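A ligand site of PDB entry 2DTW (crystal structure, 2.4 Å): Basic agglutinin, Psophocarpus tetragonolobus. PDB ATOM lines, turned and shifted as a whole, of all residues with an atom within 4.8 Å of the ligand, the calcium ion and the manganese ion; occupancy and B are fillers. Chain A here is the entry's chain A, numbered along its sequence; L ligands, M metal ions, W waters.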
ATOM      1  N   HIS A  84      20.331 -15.721  23.304  1.00  0.00           N
ATOM      2  CA  HIS A  84      21.159 -16.559  22.434  1.00  0.00           C
ATOM      3  C   HIS A  84      22.167 -15.763  21.608  1.00  0.00           C
ATOM      4  O   HIS A  84      21.823 -14.754  20.976  1.00  0.00           O
ATOM      5  CB  HIS A  84      20.247 -17.354  21.493  1.00  0.00           C
ATOM      6  CG  HIS A  84      19.217 -16.516  20.803  1.00  0.00           C
ATOM      7  ND1 HIS A  84      17.881 -16.559  21.130  1.00  0.00           N
ATOM      8  CD2 HIS A  84      19.336 -15.579  19.834  1.00  0.00           C
ATOM      9  CE1 HIS A  84      17.218 -15.682  20.401  1.00  0.00           C
ATOM     10  NE2 HIS A  84      18.080 -15.077  19.600  1.00  0.00           N
ATOM     11  N   ALA A  86      24.793 -14.910  18.479  1.00  0.00           N
ATOM     12  CA  ALA A  86      24.700 -15.060  17.017  1.00  0.00           C
ATOM     13  C   ALA A  86      25.805 -14.211  16.377  1.00  0.00           C
ATOM     14  O   ALA A  86      26.297 -13.282  17.011  1.00  0.00           O
ATOM     15  CB  ALA A  86      23.322 -14.604  16.531  1.00  0.00           C
ATOM     16  N   ASP A  87      26.232 -14.551  15.163  1.00  0.00           N
ATOM     17  CA  ASP A  87      25.727 -15.712  14.428  1.00  0.00           C
ATOM     18  C   ASP A  87      26.836 -16.739  14.155  1.00  0.00           C
ATOM     19  O   ASP A  87      26.564 -17.921  14.001  1.00  0.00           O
ATOM     20  CB  ASP A  87      25.123 -15.281  13.085  1.00  0.00           C
ATOM     21  CG  ASP A  87      23.675 -14.894  13.213  1.00  0.00           C
ATOM     22  OD1 ASP A  87      23.398 -13.699  13.489  1.00  0.00           O
ATOM     23  OD2 ASP A  87      22.814 -15.793  13.058  1.00  0.00           O
ATOM     24  N   GLY A 104      23.263 -11.933   9.473  1.00  0.00           N
ATOM     25  CA  GLY A 104      22.618 -12.979  10.242  1.00  0.00           C
ATOM     26  C   GLY A 104      23.127 -14.369   9.924  1.00  0.00           C
ATOM     27  O   GLY A 104      24.340 -14.583   9.766  1.00  0.00           O
ATOM     28  N   GLY A 105      22.211 -15.328   9.819  1.00  0.00           N
ATOM     29  CA  GLY A 105      22.591 -16.703   9.514  1.00  0.00           C
ATOM     30  C   GLY A 105      23.279 -16.930   8.183  1.00  0.00           C
ATOM     31  O   GLY A 105      23.730 -18.038   7.917  1.00  0.00           O
ATOM     32  N   PHE A 107      25.923 -15.206   7.341  1.00  0.00           N
ATOM     33  CA  PHE A 107      27.311 -14.854   7.614  1.00  0.00           C
ATOM     34  C   PHE A 107      27.932 -13.765   6.749  1.00  0.00           C
ATOM     35  O   PHE A 107      29.111 -13.461   6.902  1.00  0.00           O
ATOM     36  CB  PHE A 107      28.182 -16.106   7.494  1.00  0.00           C
ATOM     37  CG  PHE A 107      27.721 -17.256   8.356  1.00  0.00           C
ATOM     38  CD1 PHE A 107      27.738 -17.162   9.738  1.00  0.00           C
ATOM     39  CD2 PHE A 107      27.304 -18.443   7.768  1.00  0.00           C
ATOM     40  CE1 PHE A 107      27.340 -18.245  10.541  1.00  0.00           C
ATOM     41  CE2 PHE A 107      26.901 -19.534   8.549  1.00  0.00           C
ATOM     42  CZ  PHE A 107      26.925 -19.445   9.935  1.00  0.00           C
ATOM     43  N   GLU A 122      32.065 -23.241   8.329  1.00  0.00           N
ATOM     44  CA  GLU A 122      31.421 -22.373   9.291  1.00  0.00           C
ATOM     45  C   GLU A 122      31.560 -22.849  10.725  1.00  0.00           C
ATOM     46  O   GLU A 122      31.675 -24.035  11.010  1.00  0.00           O
ATOM     47  CB  GLU A 122      29.921 -22.260   8.986  1.00  0.00           C
ATOM     48  CG  GLU A 122      29.201 -23.586   9.084  1.00  0.00           C
ATOM     49  CD  GLU A 122      27.685 -23.466   9.066  1.00  0.00           C
ATOM     50  OE1 GLU A 122      27.139 -22.813   8.150  1.00  0.00           O
ATOM     51  OE2 GLU A 122      27.051 -24.048   9.967  1.00  0.00           O
ATOM     52  N   ASP A 124      29.238 -22.059  13.329  1.00  0.00           N
ATOM     53  CA  ASP A 124      27.896 -21.575  13.581  1.00  0.00           C
ATOM     54  C   ASP A 124      27.519 -21.540  15.051  1.00  0.00           C
ATOM     55  O   ASP A 124      27.530 -22.562  15.717  1.00  0.00           O
ATOM     56  CB  ASP A 124      26.918 -22.484  12.840  1.00  0.00           C
ATOM     57  CG  ASP A 124      25.666 -21.728  12.481  1.00  0.00           C
ATOM     58  OD1 ASP A 124      25.600 -20.484  12.703  1.00  0.00           O
ATOM     59  OD2 ASP A 124      24.736 -22.382  11.980  1.00  0.00           O
ATOM     60  N   PHE A 126      24.509 -19.737  16.131  1.00  0.00           N
ATOM     61  CA  PHE A 126      23.073 -19.515  16.270  1.00  0.00           C
ATOM     62  C   PHE A 126      22.286 -20.543  15.464  1.00  0.00           C
ATOM     63  O   PHE A 126      22.572 -20.774  14.281  1.00  0.00           O
ATOM     64  CB  PHE A 126      22.686 -18.115  15.801  1.00  0.00           C
ATOM     65  CG  PHE A 126      21.213 -17.867  15.844  1.00  0.00           C
ATOM     66  CD1 PHE A 126      20.588 -17.512  17.025  1.00  0.00           C
ATOM     67  CD2 PHE A 126      20.434 -18.071  14.699  1.00  0.00           C
ATOM     68  CE1 PHE A 126      19.193 -17.366  17.088  1.00  0.00           C
ATOM     69  CE2 PHE A 126      19.047 -17.943  14.748  1.00  0.00           C
ATOM     70  CZ  PHE A 126      18.432 -17.582  15.943  1.00  0.00           C
ATOM     71  N   ARG A 127      21.270 -21.126  16.083  1.00  0.00           N
ATOM     72  CA  ARG A 127      20.482 -22.142  15.394  1.00  0.00           C
ATOM     73  C   ARG A 127      19.338 -21.600  14.558  1.00  0.00           C
ATOM     74  O   ARG A 127      18.276 -21.276  15.073  1.00  0.00           O
ATOM     75  CB  ARG A 127      19.942 -23.165  16.393  1.00  0.00           C
ATOM     76  CG  ARG A 127      19.271 -24.335  15.707  1.00  0.00           C
ATOM     77  CD  ARG A 127      18.850 -25.427  16.668  1.00  0.00           C
ATOM     78  NE  ARG A 127      18.491 -26.653  15.947  1.00  0.00           N
ATOM     79  CZ  ARG A 127      18.082 -27.774  16.526  1.00  0.00           C
ATOM     80  NH1 ARG A 127      17.948 -27.831  17.845  1.00  0.00           N
ATOM     81  NH2 ARG A 127      17.817 -28.846  15.780  1.00  0.00           N
ATOM     82  N   ASN A 128      19.563 -21.521  13.245  1.00  0.00           N
ATOM     83  CA  ASN A 128      18.522 -21.074  12.317  1.00  0.00           C
ATOM     84  C   ASN A 128      17.592 -22.264  12.066  1.00  0.00           C
ATOM     85  O   ASN A 128      17.846 -23.366  12.546  1.00  0.00           O
ATOM     86  CB  ASN A 128      19.143 -20.624  10.995  1.00  0.00           C
ATOM     87  CG  ASN A 128      19.679 -19.196  11.001  1.00  0.00           C
ATOM     88  OD1 ASN A 128      20.883 -18.969  11.083  1.00  0.00           O
ATOM     89  ND2 ASN A 128      18.765 -18.226  10.911  1.00  0.00           N
ATOM     90  N   TRP A 130      17.272 -24.041   9.515  1.00  0.00           N
ATOM     91  CA  TRP A 130      17.975 -25.062   8.741  1.00  0.00           C
ATOM     92  C   TRP A 130      19.151 -25.685   9.488  1.00  0.00           C
ATOM     93  O   TRP A 130      19.833 -26.548   8.932  1.00  0.00           O
ATOM     94  CB  TRP A 130      18.488 -24.440   7.447  1.00  0.00           C
ATOM     95  CG  TRP A 130      19.440 -23.290   7.706  1.00  0.00           C
ATOM     96  CD1 TRP A 130      20.728 -23.368   8.154  1.00  0.00           C
ATOM     97  CD2 TRP A 130      19.158 -21.893   7.560  1.00  0.00           C
ATOM     98  NE1 TRP A 130      21.267 -22.114   8.301  1.00  0.00           N
ATOM     99  CE2 TRP A 130      20.320 -21.191   7.938  1.00  0.00           C
ATOM    100  CE3 TRP A 130      18.029 -21.160   7.142  1.00  0.00           C
ATOM    101  CZ2 TRP A 130      20.398 -19.788   7.923  1.00  0.00           C
ATOM    102  CZ3 TRP A 130      18.101 -19.765   7.127  1.00  0.00           C
ATOM    103  CH2 TRP A 130      19.277 -19.097   7.508  1.00  0.00           C
ATOM    104  N   ASP A 131      19.393 -25.259  10.731  1.00  0.00           N
ATOM    105  CA  ASP A 131      20.522 -25.741  11.525  1.00  0.00           C
ATOM    106  C   ASP A 131      20.270 -26.842  12.528  1.00  0.00           C
ATOM    107  O   ASP A 131      19.171 -26.978  13.064  1.00  0.00           O
ATOM    108  CB  ASP A 131      21.156 -24.621  12.362  1.00  0.00           C
ATOM    109  CG  ASP A 131      21.965 -23.615  11.608  1.00  0.00           C
ATOM    110  OD1 ASP A 131      22.638 -24.006  10.639  1.00  0.00           O
ATOM    111  OD2 ASP A 131      21.943 -22.427  12.023  1.00  0.00           O
ATOM    112  N   PRO A 132      21.301 -27.651  12.808  1.00  0.00           N
ATOM    113  CA  PRO A 132      21.198 -28.732  13.785  1.00  0.00           C
ATOM    114  C   PRO A 132      21.657 -28.019  15.070  1.00  0.00           C
ATOM    115  O   PRO A 132      21.829 -26.802  15.059  1.00  0.00           O
ATOM    116  CB  PRO A 132      22.227 -29.738  13.292  1.00  0.00           C
ATOM    117  CG  PRO A 132      23.292 -28.850  12.726  1.00  0.00           C
ATOM    118  CD  PRO A 132      22.472 -27.840  11.941  1.00  0.00           C
ATOM    119  N   HIS A 136      28.228 -25.632  16.049  1.00  0.00           N
ATOM    120  CA  HIS A 136      28.653 -26.727  15.202  1.00  0.00           C
ATOM    121  C   HIS A 136      29.553 -26.253  14.086  1.00  0.00           C
ATOM    122  O   HIS A 136      29.506 -25.099  13.681  1.00  0.00           O
ATOM    123  CB  HIS A 136      27.451 -27.483  14.604  1.00  0.00           C
ATOM    124  CG  HIS A 136      26.525 -26.655  13.779  1.00  0.00           C
ATOM    125  ND1 HIS A 136      25.402 -26.058  14.292  1.00  0.00           N
ATOM    126  CD2 HIS A 136      26.530 -26.352  12.451  1.00  0.00           C
ATOM    127  CE1 HIS A 136      24.746 -25.426  13.331  1.00  0.00           C
ATOM    128  NE2 HIS A 136      25.416 -25.595  12.208  1.00  0.00           N
ATOM    129  N   VAL A 144      24.181 -22.270   2.856  1.00  0.00           N
ATOM    130  CA  VAL A 144      24.476 -22.296   4.282  1.00  0.00           C
ATOM    131  C   VAL A 144      23.891 -23.551   4.916  1.00  0.00           C
ATOM    132  O   VAL A 144      24.010 -23.768   6.126  1.00  0.00           O
ATOM    133  CB  VAL A 144      23.913 -21.018   4.979  1.00  0.00           C
ATOM    134  CG1 VAL A 144      24.666 -19.796   4.535  1.00  0.00           C
ATOM    135  CG2 VAL A 144      22.444 -20.853   4.606  1.00  0.00           C
ATOM    136  N   SER A 146      24.609 -26.818   5.400  1.00  0.00           N
ATOM    137  CA  SER A 146      25.775 -27.704   5.377  1.00  0.00           C
ATOM    138  C   SER A 146      25.553 -29.111   4.837  1.00  0.00           C
ATOM    139  O   SER A 146      24.500 -29.713   5.054  1.00  0.00           O
ATOM    140  CB  SER A 146      26.370 -27.814   6.780  1.00  0.00           C
ATOM    141  OG  SER A 146      26.690 -26.548   7.302  1.00  0.00           O
ATOM    142  N   THR A 210      26.718 -10.762  13.356  1.00  0.00           N
ATOM    143  CA  THR A 210      26.061 -10.810  14.645  1.00  0.00           C
ATOM    144  C   THR A 210      24.565 -10.737  14.405  1.00  0.00           C
ATOM    145  O   THR A 210      24.128 -10.545  13.258  1.00  0.00           O
ATOM    146  CB  THR A 210      26.502  -9.655  15.566  1.00  0.00           C
ATOM    147  OG1 THR A 210      26.271  -8.409  14.907  1.00  0.00           O
ATOM    148  CG2 THR A 210      27.986  -9.795  15.917  1.00  0.00           C
ATOM    149  N   GLY A 211      23.783 -10.892  15.466  1.00  0.00           N
ATOM    150  CA  GLY A 211      22.334 -10.889  15.369  1.00  0.00           C
ATOM    151  C   GLY A 211      21.671  -9.913  14.420  1.00  0.00           C
ATOM    152  O   GLY A 211      21.985  -8.720  14.411  1.00  0.00           O
ATOM    153  N   ASP A 212      20.743 -10.418  13.610  1.00  0.00           N
ATOM    154  CA  ASP A 212      20.026  -9.562  12.681  1.00  0.00           C
ATOM    155  C   ASP A 212      18.943  -8.802  13.454  1.00  0.00           C
ATOM    156  O   ASP A 212      18.308  -9.347  14.357  1.00  0.00           O
ATOM    157  CB  ASP A 212      19.350 -10.371  11.579  1.00  0.00           C
ATOM    158  CG  ASP A 212      18.728  -9.470  10.532  1.00  0.00           C
ATOM    159  OD1 ASP A 212      19.354  -9.281   9.460  1.00  0.00           O
ATOM    160  OD2 ASP A 212      17.634  -8.951  10.790  1.00  0.00           O
ATOM    161  N   SER A 214      15.971  -8.097  12.791  1.00  0.00           N
ATOM    162  CA  SER A 214      14.672  -8.757  12.724  1.00  0.00           C
ATOM    163  C   SER A 214      14.422  -9.727  13.871  1.00  0.00           C
ATOM    164  O   SER A 214      13.276 -10.083  14.158  1.00  0.00           O
ATOM    165  CB  SER A 214      14.507  -9.489  11.387  1.00  0.00           C
ATOM    166  OG  SER A 214      15.314 -10.651  11.330  1.00  0.00           O
ATOM    167  N   GLY A 215      15.496 -10.158  14.534  1.00  0.00           N
ATOM    168  CA  GLY A 215      15.353 -11.080  15.644  1.00  0.00           C
ATOM    169  C   GLY A 215      14.924 -10.350  16.894  1.00  0.00           C
ATOM    170  O   GLY A 215      14.586 -10.954  17.910  1.00  0.00           O
ATOM    171  N   GLN A 217      16.487  -8.951  19.141  1.00  0.00           N
ATOM    172  CA  GLN A 217      17.285  -9.198  20.336  1.00  0.00           C
ATOM    173  C   GLN A 217      18.682  -8.591  20.201  1.00  0.00           C
ATOM    174  O   GLN A 217      19.516  -9.059  19.429  1.00  0.00           O
ATOM    175  CB  GLN A 217      17.394 -10.708  20.609  1.00  0.00           C
ATOM    176  CG  GLN A 217      16.107 -11.334  21.107  1.00  0.00           C
ATOM    177  CD  GLN A 217      15.541 -10.619  22.321  1.00  0.00           C
ATOM    178  OE1 GLN A 217      15.007  -9.522  22.209  1.00  0.00           O
ATOM    179  NE2 GLN A 217      15.660 -11.236  23.486  1.00  0.00           N
ATOM    180  N   ALA A 220      21.824 -10.773  20.944  1.00  0.00           N
ATOM    181  CA  ALA A 220      22.234 -11.784  19.984  1.00  0.00           C
ATOM    182  C   ALA A 220      23.517 -11.335  19.288  1.00  0.00           C
ATOM    183  O   ALA A 220      23.505 -10.950  18.120  1.00  0.00           O
ATOM    184  CB  ALA A 220      21.147 -12.021  18.975  1.00  0.00           C
HETATM  185  C1  LIG L   1      17.222 -13.658  13.032  1.00  0.00           C
HETATM  186  C2  LIG L   1      18.376 -14.246  12.101  1.00  0.00           C
HETATM  187  C3  LIG L   1      19.295 -15.228  12.938  1.00  0.00           C
HETATM  188  C4  LIG L   1      19.877 -14.465  14.181  1.00  0.00           C
HETATM  189  C5  LIG L   1      18.694 -13.929  15.048  1.00  0.00           C
HETATM  190  C6  LIG L   1      19.200 -13.162  16.240  1.00  0.00           C
HETATM  191  C7  LIG L   1      18.484 -14.960   9.658  1.00  0.00           C
HETATM  192  O1  LIG L   1      16.280 -14.677  13.422  1.00  0.00           O
HETATM  193  O2  LIG L   1      17.805 -14.896  10.934  1.00  0.00           O
HETATM  194  O3  LIG L   1      20.321 -15.742  12.118  1.00  0.00           O
HETATM  195  O4  LIG L   1      20.743 -13.405  13.763  1.00  0.00           O
HETATM  196  O5  LIG L   1      17.837 -13.027  14.242  1.00  0.00           O
HETATM  197  O6  LIG L   1      18.119 -12.670  17.034  1.00  0.00           O
HETATM  198 CA    CA M   1      23.175 -20.446  11.966  1.00  0.00          CA
HETATM  199 MN    MN M   2      24.854 -24.121  10.499  1.00  0.00          MN
HETATM  200  O   HOH W   1      24.503 -22.754   8.729  1.00  0.00           O
HETATM  201  O   HOH W   2      23.684 -20.283   9.612  1.00  0.00           O
HETATM  202  O   HOH W   3      24.902 -25.934   9.129  1.00  0.00           O
HETATM  203  O   HOH W   4      23.863 -18.242  12.397  1.00  0.00           O
HETATM  204  O   HOH W   5      18.353  -9.942  16.953  1.00  0.00           O
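Residues that only touch the ligand: His 84 (3.5 Å), Ala 86 (3.97 Å), Gly 104 (3.8 Å), Gly 211 (3.4 Å), Ser 214 (3.9 Å), Gly 215 (3.5 Å) and Ala 220 (3.5 Å).
Within 4 Å of the ligand: His 84, Ala 86, Asp 87, Gly 104, Gly 105, Phe 126, Asn 128, Gly 211, Asp 212, Ser 214, Gly 215 and Ala 220.
The nearest printed residue that does not touch the ligand is Gln 217 (4.1 Å).
Of the 24 residues printed, 4 come within 4 Å of the manganese ion.
The nearest printed residue that does not touch the manganese ion is Ser 146 (4.4 Å).
Water W2 lies within hydrogen-bond range of O of Gly 105 (2.8 Å) and NE1 of Trp 130 (3.3 Å).
Water W1 lies within hydrogen-bond range of OE1 of Glu 122 (2.7 Å), O of Val 144 (2.8 Å) and NE1 of Trp 130 (3.3 Å).
Water W5 lies within hydrogen-bond range of the backbone carbonyl oxygen (O) of Asp 212 (2.7 Å), an oxygen (O6) of the ligand (2.7 Å) and the backbone carbonyl oxygen (O) of Gln 217 (2.9 Å).
The side-chain carboxylate (OD2) of Asp 212 is in hydrogen-bond range of the backbone NH (N) of Ser 214, 2.7 Å away.
O of Asp 131 lies within hydrogen-bond range of NE of Arg 127, 3.0 Å away.
N of Gly 211 is in hydrogen-bond range of O of Ala 220 (2.7 Å).
N of Phe 126 is in hydrogen-bond range of O of Asp 87 (3.5 Å).
N of Gly 105 lies within hydrogen-bond range of OD2 of Asp 87 (3.3 Å).
The side-chain carboxylate (OD1) of Asp 131 lies close to the indole nitrogen (NE1) of Trp 130, at 3.3 Å.
The side-chain carboxylate of Asp 87 lies within hydrogen-bond range of the backbone NH of Gly 211, at 3.5 Å.
N of Gly 105 sits at hydrogen-bond distance from O3 of the ligand (3.0 Å).
The side-chain carboxylate (OD2) of Asp 87 sits at hydrogen-bond distance from an oxygen (O3) of the ligand, 2.7 Å away.
ND2 of Asn 128 sits at hydrogen-bond distance from O3 of the ligand.
N of Asp 212 is in hydrogen-bond range of O4 of the ligand (3.0 Å).
Four residues have an atom within 4 Å of the calcium ion: Asp 124, Phe 126, Asn 128 and Asp 131.
The manganese ion is bound by the side-chain carboxylate (OD1) of Asp 131, 2.2 Å away.
OE2 of Glu 122 binds the manganese ion, at 2.3 Å.
Water W1 binds the manganese ion.
Water W3 binds the manganese ion, 2.3 Å away.
The side-chain carboxylate (OD2) of Asp 124 is bound to the manganese ion (2.3 Å).
A ring nitrogen (NE2) of His 136 binds the manganese ion.
The manganese ion has six donor atoms within binding distance.
OD2 of Asp 131 is bound to the calcium ion (2.3 Å).
Water W4 is bound to the calcium ion.
Water W2 binds the calcium ion (2.4 Å).
The backbone carbonyl oxygen (O) of Phe 126 binds the calcium ion, at 2.4 Å.
The side-chain carboxylate (OD2) of Asp 124 is bound to the calcium ion (2.5 Å).
The side-chain carboxylate (OD1) of Asp 124 is bound to the calcium ion.
The calcium ion is bound by OD1 of Asn 128.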
